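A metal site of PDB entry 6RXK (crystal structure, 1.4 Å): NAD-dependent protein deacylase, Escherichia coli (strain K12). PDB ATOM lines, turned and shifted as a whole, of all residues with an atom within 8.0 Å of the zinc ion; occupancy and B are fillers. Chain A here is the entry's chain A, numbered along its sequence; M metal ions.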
ATOM      1  N   ARG A 129       2.881 -11.327   4.294  1.00  0.00           N
ATOM      2  CA  ARG A 129       2.263 -11.425   5.611  1.00  0.00           C
ATOM      3  C   ARG A 129       1.237 -12.531   5.580  1.00  0.00           C
ATOM      4  O   ARG A 129       0.436 -12.623   4.643  1.00  0.00           O
ATOM      5  CB  ARG A 129       1.561 -10.080   5.942  1.00  0.00           C
ATOM      6  CG  ARG A 129       1.055  -9.909   7.346  1.00  0.00           C
ATOM      7  CD  ARG A 129       0.077  -8.760   7.408  1.00  0.00           C
ATOM      8  NE  ARG A 129       0.714  -7.548   6.966  1.00  0.00           N
ATOM      9  CZ  ARG A 129       0.057  -6.433   6.708  1.00  0.00           C
ATOM     10  NH1 ARG A 129       0.741  -5.392   6.329  1.00  0.00           N
ATOM     11  NH2 ARG A 129      -1.269  -6.376   6.859  1.00  0.00           N
ATOM     12  N   CYS A 130       1.242 -13.350   6.632  1.00  0.00           N
ATOM     13  CA  CYS A 130       0.154 -14.311   6.798  1.00  0.00           C
ATOM     14  C   CYS A 130      -1.129 -13.560   7.077  1.00  0.00           C
ATOM     15  O   CYS A 130      -1.197 -12.809   8.047  1.00  0.00           O
ATOM     16  CB  CYS A 130       0.438 -15.281   7.938  1.00  0.00           C
ATOM     17  SG  CYS A 130      -0.949 -16.411   8.240  1.00  0.00           S
ATOM     18  N   SER A 131      -2.168 -13.799   6.288  1.00  0.00           N
ATOM     19  CA  SER A 131      -3.416 -13.094   6.469  1.00  0.00           C
ATOM     20  C   SER A 131      -4.150 -13.473   7.768  1.00  0.00           C
ATOM     21  O   SER A 131      -5.071 -12.771   8.181  1.00  0.00           O
ATOM     22  CB  SER A 131      -4.327 -13.363   5.256  1.00  0.00           C
ATOM     23  OG  SER A 131      -4.632 -14.744   5.149  1.00  0.00           O
ATOM     24  N   GLN A 132      -3.733 -14.562   8.412  1.00  0.00           N
ATOM     25  CA  GLN A 132      -4.344 -15.056   9.644  1.00  0.00           C
ATOM     26  C   GLN A 132      -3.528 -14.671  10.892  1.00  0.00           C
ATOM     27  O   GLN A 132      -4.067 -14.055  11.808  1.00  0.00           O
ATOM     28  CB  GLN A 132      -4.508 -16.583   9.507  1.00  0.00           C
ATOM     29  CG  GLN A 132      -5.175 -17.379  10.614  1.00  0.00           C
ATOM     30  CD  GLN A 132      -5.660 -18.732  10.078  1.00  0.00           C
ATOM     31  OE1 GLN A 132      -4.895 -19.721   9.989  1.00  0.00           O
ATOM     32  NE2 GLN A 132      -6.923 -18.769   9.657  1.00  0.00           N
ATOM     33  N   SER A 133      -2.251 -15.017  10.907  1.00  0.00           N
ATOM     34  CA  SER A 133      -1.411 -14.784  12.095  1.00  0.00           C
ATOM     35  C   SER A 133      -0.793 -13.383  12.115  1.00  0.00           C
ATOM     36  O   SER A 133      -0.416 -12.888  13.189  1.00  0.00           O
ATOM     37  CB  SER A 133      -0.274 -15.808  12.178  1.00  0.00           C
ATOM     38  OG  SER A 133       0.774 -15.482  11.260  1.00  0.00           O
ATOM     39  N   GLY A 134      -0.664 -12.755  10.945  1.00  0.00           N
ATOM     40  CA  GLY A 134       0.087 -11.513  10.848  1.00  0.00           C
ATOM     41  C   GLY A 134       1.595 -11.665  10.806  1.00  0.00           C
ATOM     42  O   GLY A 134       2.310 -10.671  10.721  1.00  0.00           O
ATOM     43  N   GLN A 135       2.118 -12.881  10.842  1.00  0.00           N
ATOM     44  CA  GLN A 135       3.556 -13.093  10.778  1.00  0.00           C
ATOM     45  C   GLN A 135       4.081 -12.677   9.404  1.00  0.00           C
ATOM     46  O   GLN A 135       3.414 -12.886   8.381  1.00  0.00           O
ATOM     47  CB  GLN A 135       3.927 -14.536  11.127  1.00  0.00           C
ATOM     48  CG  GLN A 135       3.710 -14.793  12.610  1.00  0.00           C
ATOM     49  CD  GLN A 135       4.053 -16.195  13.021  1.00  0.00           C
ATOM     50  OE1 GLN A 135       5.005 -16.786  12.510  1.00  0.00           O
ATOM     51  NE2 GLN A 135       3.291 -16.734  13.967  1.00  0.00           N
ATOM     52  N   LEU A 137       7.114 -12.552   6.434  1.00  0.00           N
ATOM     53  CA  LEU A 137       8.120 -13.368   5.801  1.00  0.00           C
ATOM     54  C   LEU A 137       8.877 -12.549   4.765  1.00  0.00           C
ATOM     55  O   LEU A 137       8.240 -11.789   4.040  1.00  0.00           O
ATOM     56  CB  LEU A 137       7.458 -14.523   5.038  1.00  0.00           C
ATOM     57  CG  LEU A 137       6.711 -15.603   5.806  1.00  0.00           C
ATOM     58  CD1 LEU A 137       5.964 -16.486   4.804  1.00  0.00           C
ATOM     59  CD2 LEU A 137       7.678 -16.424   6.651  1.00  0.00           C
ATOM     60  N   LYS A 148       0.702 -20.478   0.592  1.00  0.00           N
ATOM     61  CA  LYS A 148       0.064 -20.289   1.875  1.00  0.00           C
ATOM     62  C   LYS A 148       1.154 -20.192   2.919  1.00  0.00           C
ATOM     63  O   LYS A 148       2.300 -20.562   2.670  1.00  0.00           O
ATOM     64  CB  LYS A 148      -0.843 -21.470   2.199  1.00  0.00           C
ATOM     65  CG  LYS A 148      -1.884 -21.786   1.134  1.00  0.00           C
ATOM     66  CD  LYS A 148      -3.224 -21.179   1.467  1.00  0.00           C
ATOM     67  CE  LYS A 148      -4.340 -21.875   0.690  1.00  0.00           C
ATOM     68  NZ  LYS A 148      -4.448 -21.412  -0.709  1.00  0.00           N
ATOM     69  N   CYS A 149       0.779 -19.724   4.100  1.00  0.00           N
ATOM     70  CA  CYS A 149       1.715 -19.539   5.205  1.00  0.00           C
ATOM     71  C   CYS A 149       2.297 -20.875   5.703  1.00  0.00           C
ATOM     72  O   CYS A 149       1.784 -21.944   5.394  1.00  0.00           O
ATOM     73  CB  CYS A 149       0.994 -18.828   6.331  1.00  0.00           C
ATOM     74  SG  CYS A 149      -0.002 -19.921   7.385  1.00  0.00           S
ATOM     75  N   HIS A 150       3.362 -20.785   6.472  1.00  0.00           N
ATOM     76  CA  HIS A 150       3.840 -21.969   7.206  1.00  0.00           C
ATOM     77  C   HIS A 150       3.752 -21.746   8.709  1.00  0.00           C
ATOM     78  O   HIS A 150       4.313 -22.520   9.478  1.00  0.00           O
ATOM     79  CB  HIS A 150       5.255 -22.371   6.780  1.00  0.00           C
ATOM     80  CG  HIS A 150       6.244 -21.256   6.777  1.00  0.00           C
ATOM     81  ND1 HIS A 150       6.567 -20.549   5.631  1.00  0.00           N
ATOM     82  CD2 HIS A 150       7.016 -20.740   7.769  1.00  0.00           C
ATOM     83  CE1 HIS A 150       7.487 -19.651   5.925  1.00  0.00           C
ATOM     84  NE2 HIS A 150       7.765 -19.741   7.212  1.00  0.00           N
ATOM     85  N   CYS A 151       3.022 -20.717   9.144  1.00  0.00           N
ATOM     86  CA  CYS A 151       2.925 -20.383  10.559  1.00  0.00           C
ATOM     87  C   CYS A 151       1.640 -20.865  11.253  1.00  0.00           C
ATOM     88  O   CYS A 151       1.542 -20.749  12.474  1.00  0.00           O
ATOM     89  CB  CYS A 151       3.079 -18.879  10.768  1.00  0.00           C
ATOM     90  SG  CYS A 151       2.061 -17.808   9.674  1.00  0.00           S
ATOM     91  N   CYS A 152       0.672 -21.353  10.497  1.00  0.00           N
ATOM     92  CA  CYS A 152      -0.624 -21.734  11.034  1.00  0.00           C
ATOM     93  C   CYS A 152      -0.902 -23.207  10.766  1.00  0.00           C
ATOM     94  O   CYS A 152      -0.573 -23.745   9.716  1.00  0.00           O
ATOM     95  CB  CYS A 152      -1.768 -20.923  10.384  1.00  0.00           C
ATOM     96  SG  CYS A 152      -1.612 -19.159  10.678  1.00  0.00           S
ATOM     97  N   GLN A 153      -1.586 -23.839  11.725  1.00  0.00           N
ATOM     98  CA  GLN A 153      -2.004 -25.207  11.548  1.00  0.00           C
ATOM     99  C   GLN A 153      -2.880 -25.346  10.337  1.00  0.00           C
ATOM    100  O   GLN A 153      -2.713 -26.277   9.575  1.00  0.00           O
ATOM    101  CB  GLN A 153      -2.729 -25.664  12.821  1.00  0.00           C
ATOM    102  CG  GLN A 153      -3.360 -27.016  12.634  1.00  0.00           C
ATOM    103  CD  GLN A 153      -3.909 -27.605  13.933  1.00  0.00           C
ATOM    104  OE1 GLN A 153      -3.381 -27.374  15.011  1.00  0.00           O
ATOM    105  NE2 GLN A 153      -4.983 -28.374  13.818  1.00  0.00           N
ATOM    106  N   PHE A 154      -3.777 -24.389  10.157  1.00  0.00           N
ATOM    107  CA  PHE A 154      -4.618 -24.315   8.982  1.00  0.00           C
ATOM    108  C   PHE A 154      -4.036 -23.230   8.080  1.00  0.00           C
ATOM    109  O   PHE A 154      -4.274 -22.053   8.334  1.00  0.00           O
ATOM    110  CB  PHE A 154      -6.025 -23.949   9.411  1.00  0.00           C
ATOM    111  CG  PHE A 154      -6.672 -24.984  10.292  1.00  0.00           C
ATOM    112  CD1 PHE A 154      -7.294 -26.080   9.720  1.00  0.00           C
ATOM    113  CD2 PHE A 154      -6.634 -24.883  11.674  1.00  0.00           C
ATOM    114  CE1 PHE A 154      -7.902 -27.048  10.526  1.00  0.00           C
ATOM    115  CE2 PHE A 154      -7.241 -25.842  12.485  1.00  0.00           C
ATOM    116  CZ  PHE A 154      -7.860 -26.920  11.897  1.00  0.00           C
ATOM    117  N   PRO A 155      -3.282 -23.621   7.046  1.00  0.00           N
ATOM    118  CA  PRO A 155      -2.518 -22.605   6.314  1.00  0.00           C
ATOM    119  C   PRO A 155      -3.405 -21.551   5.684  1.00  0.00           C
ATOM    120  O   PRO A 155      -4.468 -21.822   5.146  1.00  0.00           O
ATOM    121  CB  PRO A 155      -1.779 -23.396   5.256  1.00  0.00           C
ATOM    122  CG  PRO A 155      -1.655 -24.784   5.844  1.00  0.00           C
ATOM    123  CD  PRO A 155      -2.933 -24.978   6.612  1.00  0.00           C
ATOM    124  N   ALA A 156      -2.914 -20.321   5.738  1.00  0.00           N
ATOM    125  CA  ALA A 156      -3.705 -19.164   5.356  1.00  0.00           C
ATOM    126  C   ALA A 156      -3.046 -18.465   4.152  1.00  0.00           C
ATOM    127  O   ALA A 156      -1.842 -18.573   3.949  1.00  0.00           O
ATOM    128  CB  ALA A 156      -3.795 -18.211   6.511  1.00  0.00           C
ATOM    129  N   PRO A 157      -3.854 -17.761   3.352  1.00  0.00           N
ATOM    130  CA  PRO A 157      -3.282 -16.999   2.244  1.00  0.00           C
ATOM    131  C   PRO A 157      -2.301 -15.921   2.706  1.00  0.00           C
ATOM    132  O   PRO A 157      -2.382 -15.395   3.816  1.00  0.00           O
ATOM    133  CB  PRO A 157      -4.498 -16.325   1.615  1.00  0.00           C
ATOM    134  CG  PRO A 157      -5.654 -17.118   2.049  1.00  0.00           C
ATOM    135  CD  PRO A 157      -5.314 -17.612   3.413  1.00  0.00           C
ATOM    136  N   LEU A 158      -1.351 -15.648   1.827  1.00  0.00           N
ATOM    137  CA  LEU A 158      -0.352 -14.609   2.067  1.00  0.00           C
ATOM    138  C   LEU A 158      -0.772 -13.373   1.305  1.00  0.00           C
ATOM    139  O   LEU A 158      -1.316 -13.455   0.201  1.00  0.00           O
ATOM    140  CB  LEU A 158       1.003 -15.058   1.568  1.00  0.00           C
ATOM    141  CG  LEU A 158       1.585 -16.293   2.248  1.00  0.00           C
ATOM    142  CD1 LEU A 158       2.843 -16.744   1.568  1.00  0.00           C
ATOM    143  CD2 LEU A 158       1.847 -16.028   3.724  1.00  0.00           C
HETATM  144 ZN    ZN M   1      -0.172 -18.399   9.133  1.00  0.00          ZN
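The side-chain amide oxygen (OE1) of Gln 132 sits close to the side-chain sulfur (SG) of Cys 152, 3.4 Å away. The side-chain sulfur (SG) of Cys 130 lies close to the backbone NH (N) of Ser 133 (3.3 Å). The backbone NH (N) of Gln 132 sits close to the side-chain sulfur (SG) of Cys 130, 3.3 Å away. N of Cys 130 is in hydrogen-bond range of O of Gln 135, at 2.8 Å. O of Ala 156 lies within hydrogen-bond range of N of Cys 149, at 2.9 Å. The side-chain sulfur (SG) of Cys 151 lies close to the side-chain hydroxyl (OG) of Ser 133 (3.1 Å). OG of Ser 133 sits at hydrogen-bond distance from N of Gln 135 (3.0 Å).
Residues that only touch the zinc ion: Ser 133 (3.7 Å). Five residues have an atom within 4 Å of the zinc ion: Cys 130, Ser 133, Cys 149, Cys 151 and Cys 152.
The zinc ion is bound by SG of Cys 152 (2.2 Å), SG of Cys 130 (2.3 Å), SG of Cys 149 (2.3 Å) and SG of Cys 151 (2.4 Å).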
